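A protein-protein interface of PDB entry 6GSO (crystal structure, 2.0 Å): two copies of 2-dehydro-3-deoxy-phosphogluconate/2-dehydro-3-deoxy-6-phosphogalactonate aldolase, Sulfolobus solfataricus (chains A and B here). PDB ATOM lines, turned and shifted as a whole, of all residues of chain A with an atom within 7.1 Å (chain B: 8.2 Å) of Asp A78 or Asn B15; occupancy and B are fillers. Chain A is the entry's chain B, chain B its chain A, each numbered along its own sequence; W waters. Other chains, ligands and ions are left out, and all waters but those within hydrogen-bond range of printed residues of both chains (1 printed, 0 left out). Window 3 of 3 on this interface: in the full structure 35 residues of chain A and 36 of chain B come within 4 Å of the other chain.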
ATOM      1  N   LEU A  75     -12.184 -15.247  12.082  1.00  0.00           N
ATOM      2  CA  LEU A  75     -11.745 -13.987  11.507  1.00  0.00           C
ATOM      3  C   LEU A  75     -11.506 -12.921  12.565  1.00  0.00           C
ATOM      4  O   LEU A  75     -11.404 -11.728  12.239  1.00  0.00           O
ATOM      5  CB  LEU A  75     -12.759 -13.496  10.471  1.00  0.00           C
ATOM      6  CG  LEU A  75     -12.913 -14.389   9.234  1.00  0.00           C
ATOM      7  CD1 LEU A  75     -13.943 -13.806   8.241  1.00  0.00           C
ATOM      8  CD2 LEU A  75     -11.552 -14.582   8.555  1.00  0.00           C
ATOM      9  N   ASN A  76     -11.395 -13.322  13.823  1.00  0.00           N
ATOM     10  CA  ASN A  76     -10.946 -12.421  14.873  1.00  0.00           C
ATOM     11  C   ASN A  76      -9.902 -13.188  15.657  1.00  0.00           C
ATOM     12  O   ASN A  76     -10.230 -14.114  16.404  1.00  0.00           O
ATOM     13  CB  ASN A  76     -12.101 -11.950  15.761  1.00  0.00           C
ATOM     14  CG  ASN A  76     -11.630 -11.086  16.911  1.00  0.00           C
ATOM     15  OD1 ASN A  76     -10.745 -11.466  17.658  1.00  0.00           O
ATOM     16  ND2 ASN A  76     -12.205  -9.918  17.042  1.00  0.00           N
ATOM     17  N   LEU A  77      -8.645 -12.805  15.474  1.00  0.00           N
ATOM     18  CA  LEU A  77      -7.552 -13.572  16.056  1.00  0.00           C
ATOM     19  C   LEU A  77      -7.602 -13.563  17.580  1.00  0.00           C
ATOM     20  O   LEU A  77      -7.152 -14.527  18.220  1.00  0.00           O
ATOM     21  CB  LEU A  77      -6.213 -13.030  15.551  1.00  0.00           C
ATOM     22  CG  LEU A  77      -4.973 -13.717  16.104  1.00  0.00           C
ATOM     23  CD1 LEU A  77      -5.074 -15.212  15.960  1.00  0.00           C
ATOM     24  CD2 LEU A  77      -3.798 -13.173  15.355  1.00  0.00           C
ATOM     25  N   ASP A  78      -8.153 -12.501  18.181  1.00  0.00           N
ATOM     26  CA  ASP A  78      -8.266 -12.451  19.641  1.00  0.00           C
ATOM     27  C   ASP A  78      -9.155 -13.578  20.155  1.00  0.00           C
ATOM     28  O   ASP A  78      -8.802 -14.294  21.101  1.00  0.00           O
ATOM     29  CB  ASP A  78      -8.812 -11.090  20.094  1.00  0.00           C
ATOM     30  CG  ASP A  78      -7.772  -9.986  20.040  1.00  0.00           C
ATOM     31  OD1 ASP A  78      -6.613 -10.268  19.694  1.00  0.00           O
ATOM     32  OD2 ASP A  78      -8.113  -8.828  20.354  1.00  0.00           O
ATOM     33  N   ASP A  79     -10.310 -13.772  19.530  1.00  0.00           N
ATOM     34  CA  ASP A  79     -11.162 -14.890  19.930  1.00  0.00           C
ATOM     35  C   ASP A  79     -10.438 -16.226  19.766  1.00  0.00           C
ATOM     36  O   ASP A  79     -10.555 -17.119  20.620  1.00  0.00           O
ATOM     37  CB  ASP A  79     -12.465 -14.869  19.123  1.00  0.00           C
ATOM     38  CG  ASP A  79     -13.309 -13.632  19.423  1.00  0.00           C
ATOM     39  OD1 ASP A  79     -13.071 -13.045  20.493  1.00  0.00           O
ATOM     40  OD2 ASP A  79     -14.172 -13.244  18.599  1.00  0.00           O
ATOM     41  N   ALA A  80      -9.687 -16.395  18.669  1.00  0.00           N
ATOM     42  CA  ALA A  80      -8.978 -17.657  18.482  1.00  0.00           C
ATOM     43  C   ALA A  80      -7.866 -17.815  19.515  1.00  0.00           C
ATOM     44  O   ALA A  80      -7.639 -18.922  20.024  1.00  0.00           O
ATOM     45  CB  ALA A  80      -8.421 -17.757  17.053  1.00  0.00           C
ATOM     46  N   ILE A  81      -7.142 -16.734  19.828  1.00  0.00           N
ATOM     47  CA  ILE A  81      -6.118 -16.834  20.869  1.00  0.00           C
ATOM     48  C   ILE A  81      -6.748 -17.240  22.191  1.00  0.00           C
ATOM     49  O   ILE A  81      -6.192 -18.051  22.941  1.00  0.00           O
ATOM     50  CB  ILE A  81      -5.365 -15.505  21.008  1.00  0.00           C
ATOM     51  CG1 ILE A  81      -4.466 -15.302  19.803  1.00  0.00           C
ATOM     52  CG2 ILE A  81      -4.594 -15.456  22.366  1.00  0.00           C
ATOM     53  CD1 ILE A  81      -3.949 -13.871  19.632  1.00  0.00           C
ATOM     54  N   ARG A  82      -7.931 -16.691  22.489  1.00  0.00           N
ATOM     55  CA  ARG A  82      -8.588 -16.957  23.766  1.00  0.00           C
ATOM     56  C   ARG A  82      -9.034 -18.411  23.867  1.00  0.00           C
ATOM     57  O   ARG A  82      -8.908 -19.033  24.928  1.00  0.00           O
ATOM     58  CB  ARG A  82      -9.781 -16.008  23.942  1.00  0.00           C
ATOM     59  CG  ARG A  82     -10.449 -16.077  25.341  1.00  0.00           C
ATOM     60  CD  ARG A  82     -11.539 -15.017  25.527  1.00  0.00           C
ATOM     61  NE  ARG A  82     -12.687 -15.212  24.632  1.00  0.00           N
ATOM     62  CZ  ARG A  82     -13.811 -15.859  24.953  1.00  0.00           C
ATOM     63  NH1 ARG A  82     -13.974 -16.392  26.162  1.00  0.00           N
ATOM     64  NH2 ARG A  82     -14.791 -15.975  24.060  1.00  0.00           N
ATOM     65  N   LEU A  83      -9.556 -18.980  22.778  1.00  0.00           N
ATOM     66  CA  LEU A  83      -9.973 -20.380  22.821  1.00  0.00           C
ATOM     67  C   LEU A  83      -8.770 -21.301  22.979  1.00  0.00           C
ATOM     68  O   LEU A  83      -8.806 -22.274  23.755  1.00  0.00           O
ATOM     69  CB  LEU A  83     -10.766 -20.709  21.555  1.00  0.00           C
ATOM     70  CG  LEU A  83     -12.105 -19.996  21.444  1.00  0.00           C
ATOM     71  CD1 LEU A  83     -12.652 -19.968  19.997  1.00  0.00           C
ATOM     72  CD2 LEU A  83     -13.113 -20.650  22.383  1.00  0.00           C
ATOM     73  N   ALA A  84      -7.684 -20.987  22.273  1.00  0.00           N
ATOM     74  CA  ALA A  84      -6.461 -21.762  22.394  1.00  0.00           C
ATOM     75  C   ALA A  84      -5.991 -21.812  23.846  1.00  0.00           C
ATOM     76  O   ALA A  84      -5.748 -22.891  24.395  1.00  0.00           O
ATOM     77  CB  ALA A  84      -5.386 -21.162  21.490  1.00  0.00           C
ATOM     78  N   PRO B  10     -12.394   1.439  10.531  1.00  0.00           N
ATOM     79  CA  PRO B  10     -11.227   1.684  11.386  1.00  0.00           C
ATOM     80  C   PRO B  10     -11.358   0.978  12.727  1.00  0.00           C
ATOM     81  O   PRO B  10     -12.412   1.008  13.372  1.00  0.00           O
ATOM     82  CB  PRO B  10     -11.242   3.209  11.554  1.00  0.00           C
ATOM     83  CG  PRO B  10     -12.639   3.546  11.537  1.00  0.00           C
ATOM     84  CD  PRO B  10     -13.305   2.599  10.542  1.00  0.00           C
ATOM     85  N   PHE B  11     -10.273   0.362  13.171  1.00  0.00           N
ATOM     86  CA  PHE B  11     -10.243  -0.228  14.499  1.00  0.00           C
ATOM     87  C   PHE B  11      -9.190   0.470  15.356  1.00  0.00           C
ATOM     88  O   PHE B  11      -8.177   0.966  14.854  1.00  0.00           O
ATOM     89  CB  PHE B  11      -9.960  -1.736  14.484  1.00  0.00           C
ATOM     90  CG  PHE B  11     -11.008  -2.558  13.754  1.00  0.00           C
ATOM     91  CD1 PHE B  11     -10.968  -2.699  12.379  1.00  0.00           C
ATOM     92  CD2 PHE B  11     -12.004  -3.212  14.456  1.00  0.00           C
ATOM     93  CE1 PHE B  11     -11.917  -3.474  11.717  1.00  0.00           C
ATOM     94  CE2 PHE B  11     -12.961  -3.976  13.803  1.00  0.00           C
ATOM     95  CZ  PHE B  11     -12.922  -4.098  12.441  1.00  0.00           C
ATOM     96  N   THR B  12      -9.470   0.528  16.654  1.00  0.00           N
ATOM     97  CA  THR B  12      -8.530   1.035  17.644  1.00  0.00           C
ATOM     98  C   THR B  12      -7.416   0.022  17.900  1.00  0.00           C
ATOM     99  O   THR B  12      -7.420  -1.096  17.386  1.00  0.00           O
ATOM    100  CB  THR B  12      -9.236   1.298  18.961  1.00  0.00           C
ATOM    101  OG1 THR B  12      -9.810   0.058  19.421  1.00  0.00           O
ATOM    102  CG2 THR B  12     -10.301   2.383  18.810  1.00  0.00           C
ATOM    103  N   LYS B  13      -6.484   0.402  18.780  1.00  0.00           N
ATOM    104  CA  LYS B  13      -5.395  -0.500  19.157  1.00  0.00           C
ATOM    105  C   LYS B  13      -5.896  -1.719  19.922  1.00  0.00           C
ATOM    106  O   LYS B  13      -5.310  -2.801  19.824  1.00  0.00           O
ATOM    107  CB  LYS B  13      -4.362   0.254  19.997  1.00  0.00           C
ATOM    108  CG  LYS B  13      -2.965  -0.349  19.932  1.00  0.00           C
ATOM    109  CD  LYS B  13      -2.000   0.344  20.884  1.00  0.00           C
ATOM    110  CE  LYS B  13      -1.275   1.506  20.213  1.00  0.00           C
ATOM    111  NZ  LYS B  13      -0.385   2.232  21.163  1.00  0.00           N
ATOM    112  N   ASP B  14      -6.939  -1.565  20.736  1.00  0.00           N
ATOM    113  CA  ASP B  14      -7.523  -2.717  21.402  1.00  0.00           C
ATOM    114  C   ASP B  14      -8.695  -3.295  20.615  1.00  0.00           C
ATOM    115  O   ASP B  14      -9.606  -3.897  21.193  1.00  0.00           O
ATOM    116  CB  ASP B  14      -7.915  -2.374  22.852  1.00  0.00           C
ATOM    117  CG  ASP B  14      -8.736  -1.118  22.960  1.00  0.00           C
ATOM    118  OD1 ASP B  14      -9.192  -0.620  21.913  1.00  0.00           O
ATOM    119  OD2 ASP B  14      -8.923  -0.623  24.089  1.00  0.00           O
ATOM    120  N   ASN B  15      -8.689  -3.136  19.296  1.00  0.00           N
ATOM    121  CA  ASN B  15      -9.491  -3.979  18.414  1.00  0.00           C
ATOM    122  C   ASN B  15     -10.981  -3.692  18.568  1.00  0.00           C
ATOM    123  O   ASN B  15     -11.802  -4.609  18.635  1.00  0.00           O
ATOM    124  CB  ASN B  15      -9.178  -5.462  18.661  1.00  0.00           C
ATOM    125  CG  ASN B  15      -9.586  -6.360  17.498  1.00  0.00           C
ATOM    126  OD1 ASN B  15      -9.808  -5.892  16.380  1.00  0.00           O
ATOM    127  ND2 ASN B  15      -9.699  -7.653  17.768  1.00  0.00           N
ATOM    128  N   ARG B  16     -11.328  -2.407  18.634  1.00  0.00           N
ATOM    129  CA  ARG B  16     -12.706  -1.954  18.628  1.00  0.00           C
ATOM    130  C   ARG B  16     -12.878  -1.005  17.462  1.00  0.00           C
ATOM    131  O   ARG B  16     -11.915  -0.413  16.973  1.00  0.00           O
ATOM    132  CB  ARG B  16     -13.087  -1.249  19.953  1.00  0.00           C
ATOM    133  CG  ARG B  16     -13.032  -2.181  21.169  1.00  0.00           C
ATOM    134  CD  ARG B  16     -13.076  -1.461  22.520  1.00  0.00           C
ATOM    135  NE  ARG B  16     -13.486  -2.383  23.588  1.00  0.00           N
ATOM    136  CZ  ARG B  16     -12.693  -2.904  24.530  1.00  0.00           C
ATOM    137  NH1 ARG B  16     -11.401  -2.603  24.604  1.00  0.00           N
ATOM    138  NH2 ARG B  16     -13.208  -3.740  25.424  1.00  0.00           N
ATOM    139  N   ILE B  17     -14.121  -0.853  17.015  1.00  0.00           N
ATOM    140  CA  ILE B  17     -14.398   0.095  15.951  1.00  0.00           C
ATOM    141  C   ILE B  17     -14.112   1.500  16.458  1.00  0.00           C
ATOM    142  O   ILE B  17     -14.613   1.914  17.514  1.00  0.00           O
ATOM    143  CB  ILE B  17     -15.846  -0.039  15.468  1.00  0.00           C
ATOM    144  CG1 ILE B  17     -16.074  -1.436  14.850  1.00  0.00           C
ATOM    145  CG2 ILE B  17     -16.162   1.064  14.452  1.00  0.00           C
ATOM    146  CD1 ILE B  17     -17.554  -1.735  14.529  1.00  0.00           C
ATOM    147  N   ASP B  18     -13.298   2.241  15.715  1.00  0.00           N
ATOM    148  CA  ASP B  18     -13.018   3.628  16.066  1.00  0.00           C
ATOM    149  C   ASP B  18     -14.117   4.485  15.449  1.00  0.00           C
ATOM    150  O   ASP B  18     -14.029   4.905  14.301  1.00  0.00           O
ATOM    151  CB  ASP B  18     -11.631   4.022  15.585  1.00  0.00           C
ATOM    152  CG  ASP B  18     -11.176   5.350  16.163  1.00  0.00           C
ATOM    153  OD1 ASP B  18     -12.013   6.263  16.232  1.00  0.00           O
ATOM    154  OD2 ASP B  18      -9.996   5.471  16.542  1.00  0.00           O
ATOM    155  N   LEU B  45     -14.395  -5.356   6.112  1.00  0.00           N
ATOM    156  CA  LEU B  45     -14.160  -6.532   6.942  1.00  0.00           C
ATOM    157  C   LEU B  45     -15.445  -6.994   7.630  1.00  0.00           C
ATOM    158  O   LEU B  45     -15.417  -7.509   8.752  1.00  0.00           O
ATOM    159  CB  LEU B  45     -13.056  -6.269   7.973  1.00  0.00           C
ATOM    160  CG  LEU B  45     -11.670  -5.836   7.487  1.00  0.00           C
ATOM    161  CD1 LEU B  45     -10.697  -5.857   8.639  1.00  0.00           C
ATOM    162  CD2 LEU B  45     -11.148  -6.704   6.319  1.00  0.00           C
ATOM    163  N   SER B  48     -15.632 -10.127   9.531  1.00  0.00           N
ATOM    164  CA  SER B  48     -14.914 -10.181  10.794  1.00  0.00           C
ATOM    165  C   SER B  48     -15.692  -9.499  11.922  1.00  0.00           C
ATOM    166  O   SER B  48     -15.268  -9.547  13.087  1.00  0.00           O
ATOM    167  CB  SER B  48     -13.538  -9.542  10.616  1.00  0.00           C
ATOM    168  OG  SER B  48     -12.864 -10.063   9.458  1.00  0.00           O
ATOM    169  N   LEU B  49     -16.862  -8.939  11.617  1.00  0.00           N
ATOM    170  CA  LEU B  49     -17.645  -8.161  12.577  1.00  0.00           C
ATOM    171  C   LEU B  49     -18.806  -8.960  13.168  1.00  0.00           C
ATOM    172  O   LEU B  49     -19.589  -9.570  12.444  1.00  0.00           O
ATOM    173  CB  LEU B  49     -18.202  -6.901  11.917  1.00  0.00           C
ATOM    174  CG  LEU B  49     -17.206  -5.933  11.292  1.00  0.00           C
ATOM    175  CD1 LEU B  49     -17.959  -4.794  10.590  1.00  0.00           C
ATOM    176  CD2 LEU B  49     -16.254  -5.438  12.384  1.00  0.00           C
ATOM    177  N   GLU B  53     -21.358  -5.330  16.085  1.00  0.00           N
ATOM    178  CA  GLU B  53     -20.408  -4.424  15.438  1.00  0.00           C
ATOM    179  C   GLU B  53     -20.930  -3.933  14.092  1.00  0.00           C
ATOM    180  O   GLU B  53     -20.742  -2.762  13.735  1.00  0.00           O
ATOM    181  CB  GLU B  53     -19.056  -5.134  15.298  1.00  0.00           C
ATOM    182  CG  GLU B  53     -18.337  -5.257  16.607  1.00  0.00           C
ATOM    183  CD  GLU B  53     -17.122  -6.127  16.556  1.00  0.00           C
ATOM    184  OE1 GLU B  53     -17.151  -7.185  15.878  1.00  0.00           O
ATOM    185  OE2 GLU B  53     -16.134  -5.752  17.214  1.00  0.00           O
ATOM    186  N   GLU B  56     -23.014  -1.094  15.063  1.00  0.00           N
ATOM    187  CA  GLU B  56     -22.238   0.085  15.421  1.00  0.00           C
ATOM    188  C   GLU B  56     -21.738   0.803  14.191  1.00  0.00           C
ATOM    189  O   GLU B  56     -21.813   2.035  14.100  1.00  0.00           O
ATOM    190  CB  GLU B  56     -21.060  -0.306  16.305  1.00  0.00           C
ATOM    191  CG  GLU B  56     -21.441  -0.751  17.692  1.00  0.00           C
ATOM    192  CD  GLU B  56     -20.323  -1.590  18.351  1.00  0.00           C
ATOM    193  OE1 GLU B  56     -20.643  -2.607  19.024  1.00  0.00           O
ATOM    194  OE2 GLU B  56     -19.125  -1.237  18.179  1.00  0.00           O
ATOM    195  N   TYR B 258      -6.187   0.789  12.767  1.00  0.00           N
ATOM    196  CA  TYR B 258      -5.706  -0.511  12.356  1.00  0.00           C
ATOM    197  C   TYR B 258      -6.822  -1.333  11.717  1.00  0.00           C
ATOM    198  O   TYR B 258      -8.014  -1.062  11.921  1.00  0.00           O
ATOM    199  CB  TYR B 258      -5.165  -1.278  13.565  1.00  0.00           C
ATOM    200  CG  TYR B 258      -4.131  -0.547  14.377  1.00  0.00           C
ATOM    201  CD1 TYR B 258      -2.784  -0.586  14.023  1.00  0.00           C
ATOM    202  CD2 TYR B 258      -4.492   0.166  15.515  1.00  0.00           C
ATOM    203  CE1 TYR B 258      -1.832   0.079  14.777  1.00  0.00           C
ATOM    204  CE2 TYR B 258      -3.547   0.834  16.270  1.00  0.00           C
ATOM    205  CZ  TYR B 258      -2.228   0.784  15.905  1.00  0.00           C
ATOM    206  OH  TYR B 258      -1.301   1.443  16.668  1.00  0.00           O
ATOM    207  N   PRO B 259      -6.471  -2.362  10.940  1.00  0.00           N
ATOM    208  CA  PRO B 259      -7.466  -3.371  10.570  1.00  0.00           C
ATOM    209  C   PRO B 259      -7.653  -4.353  11.716  1.00  0.00           C
ATOM    210  O   PRO B 259      -7.097  -4.135  12.793  1.00  0.00           O
ATOM    211  CB  PRO B 259      -6.857  -4.029   9.327  1.00  0.00           C
ATOM    212  CG  PRO B 259      -5.364  -3.690   9.375  1.00  0.00           C
ATOM    213  CD  PRO B 259      -5.115  -2.759  10.533  1.00  0.00           C
ATOM    214  N   ARG B 260      -8.455  -5.396  11.531  1.00  0.00           N
ATOM    215  CA  ARG B 260      -8.639  -6.430  12.548  1.00  0.00           C
ATOM    216  C   ARG B 260      -7.839  -7.675  12.198  1.00  0.00           C
ATOM    217  O   ARG B 260      -8.139  -8.318  11.180  1.00  0.00           O
ATOM    218  CB  ARG B 260     -10.114  -6.787  12.671  1.00  0.00           C
ATOM    219  CG  ARG B 260     -10.395  -8.001  13.535  1.00  0.00           C
ATOM    220  CD  ARG B 260     -11.854  -8.036  13.908  1.00  0.00           C
ATOM    221  NE  ARG B 260     -12.146  -7.085  14.977  1.00  0.00           N
ATOM    222  CZ  ARG B 260     -13.348  -6.904  15.525  1.00  0.00           C
ATOM    223  NH1 ARG B 260     -14.408  -7.574  15.084  1.00  0.00           N
ATOM    224  NH2 ARG B 260     -13.491  -6.042  16.527  1.00  0.00           N
ATOM    225  N   PRO B 261      -6.854  -8.073  12.995  1.00  0.00           N
ATOM    226  CA  PRO B 261      -6.110  -9.314  12.705  1.00  0.00           C
ATOM    227  C   PRO B 261      -7.037 -10.509  12.581  1.00  0.00           C
ATOM    228  O   PRO B 261      -7.876 -10.719  13.469  1.00  0.00           O
ATOM    229  CB  PRO B 261      -5.200  -9.449  13.932  1.00  0.00           C
ATOM    230  CG  PRO B 261      -4.854  -8.042  14.223  1.00  0.00           C
ATOM    231  CD  PRO B 261      -6.157  -7.275  14.015  1.00  0.00           C
ATOM    232  N   PRO B 262      -6.827 -11.407  11.579  1.00  0.00           N
ATOM    233  CA  PRO B 262      -5.602 -11.613  10.787  1.00  0.00           C
ATOM    234  C   PRO B 262      -5.425 -10.765   9.546  1.00  0.00           C
ATOM    235  O   PRO B 262      -4.515 -11.033   8.778  1.00  0.00           O
ATOM    236  CB  PRO B 262      -5.703 -13.088  10.384  1.00  0.00           C
ATOM    237  CG  PRO B 262      -7.151 -13.338  10.288  1.00  0.00           C
ATOM    238  CD  PRO B 262      -7.796 -12.500  11.359  1.00  0.00           C
ATOM    239  N   ILE B 263      -6.276  -9.775   9.323  1.00  0.00           N
ATOM    240  CA  ILE B 263      -5.968  -8.742   8.351  1.00  0.00           C
ATOM    241  C   ILE B 263      -4.979  -7.818   9.039  1.00  0.00           C
ATOM    242  O   ILE B 263      -5.383  -6.840   9.675  1.00  0.00           O
ATOM    243  CB  ILE B 263      -7.230  -7.994   7.893  1.00  0.00           C
ATOM    244  CG1 ILE B 263      -8.253  -8.984   7.316  1.00  0.00           C
ATOM    245  CG2 ILE B 263      -6.883  -6.899   6.874  1.00  0.00           C
ATOM    246  CD1 ILE B 263      -7.710  -9.838   6.179  1.00  0.00           C
HETATM  247  O   HOH W   1     -10.321 -10.147  10.470  1.00  0.00           O
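Printed residues of chain B within 4 Å of Leu A77: Pro B261.
Of chain B, only Asn B15 comes within 4 Å of Asp A78.
Asn B15 touches two residues of chain A.
Of the printed residues of chain A, Ser B48 touches Leu A75.
Tyr B258 touches none of the printed residues of chain A.
The nearest residue of chain A that does not touch Asn B15 is Leu A77 (5.7 Å).
No position is printed for both chains.
Of the 8 pairs that touch across the chains among the printed residues, none has its exchanged pair printed and touching as well.
Water W1 lies within hydrogen-bond range of O of Leu A75 (2.6 Å), OG of Ser B48 (2.7 Å) and O of Arg B260 (2.9 Å).
The side-chain amide nitrogen (ND2) of Asn A76 lies close to the side-chain amide nitrogen (ND2) of Asn B15, at 3.5 Å.
The side-chain amide nitrogen of Asn B15 sits at hydrogen-bond distance from the side-chain carboxylate of Asp A78.
The backbone NH (N) of Leu A77 is in hydrogen-bond range of the backbone carbonyl oxygen (O) of Pro B261, at 3.0 Å.
The side-chain hydroxyl (OG1) of Thr B12 is in hydrogen-bond range of the backbone NH (N) of Asn B15 (3.4 Å).
OD1 of Asn B15 lies within hydrogen-bond range of NE of Arg B260 (3.0 Å).
NH1 of Arg B260 is in hydrogen-bond range of O of Ser B48 (2.9 Å).
NH2 of Arg B260 lies within salt-bridge range of OE2 of Glu B53, 2.7 Å away.
N of Asp A78 sits at hydrogen-bond distance from OD1 of Asn A76.
The side-chain amide oxygen (OD1) of Asn A76 is in hydrogen-bond range of the backbone NH (N) of Asp A79, 3.0 Å away.
Of the 20 printed residues of chain B, 5 touch a printed residue of chain A.
Printed residues of chain B that touch a printed residue of chain A: Asn B15, Ser B48, Arg B260, Pro B261 and Pro B262.
CB of Ser B48 touches O of Leu A75, at 3.5 Å.
Leu A75 touches Pro B261 (O to O, 3.9 Å).
Pro B262 touches Leu A75.
NE of Arg B260 touches ND2 of Asn A76, 3.5 Å away.
O of Pro B261 touches CA of Asn A76, at 3.8 Å.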
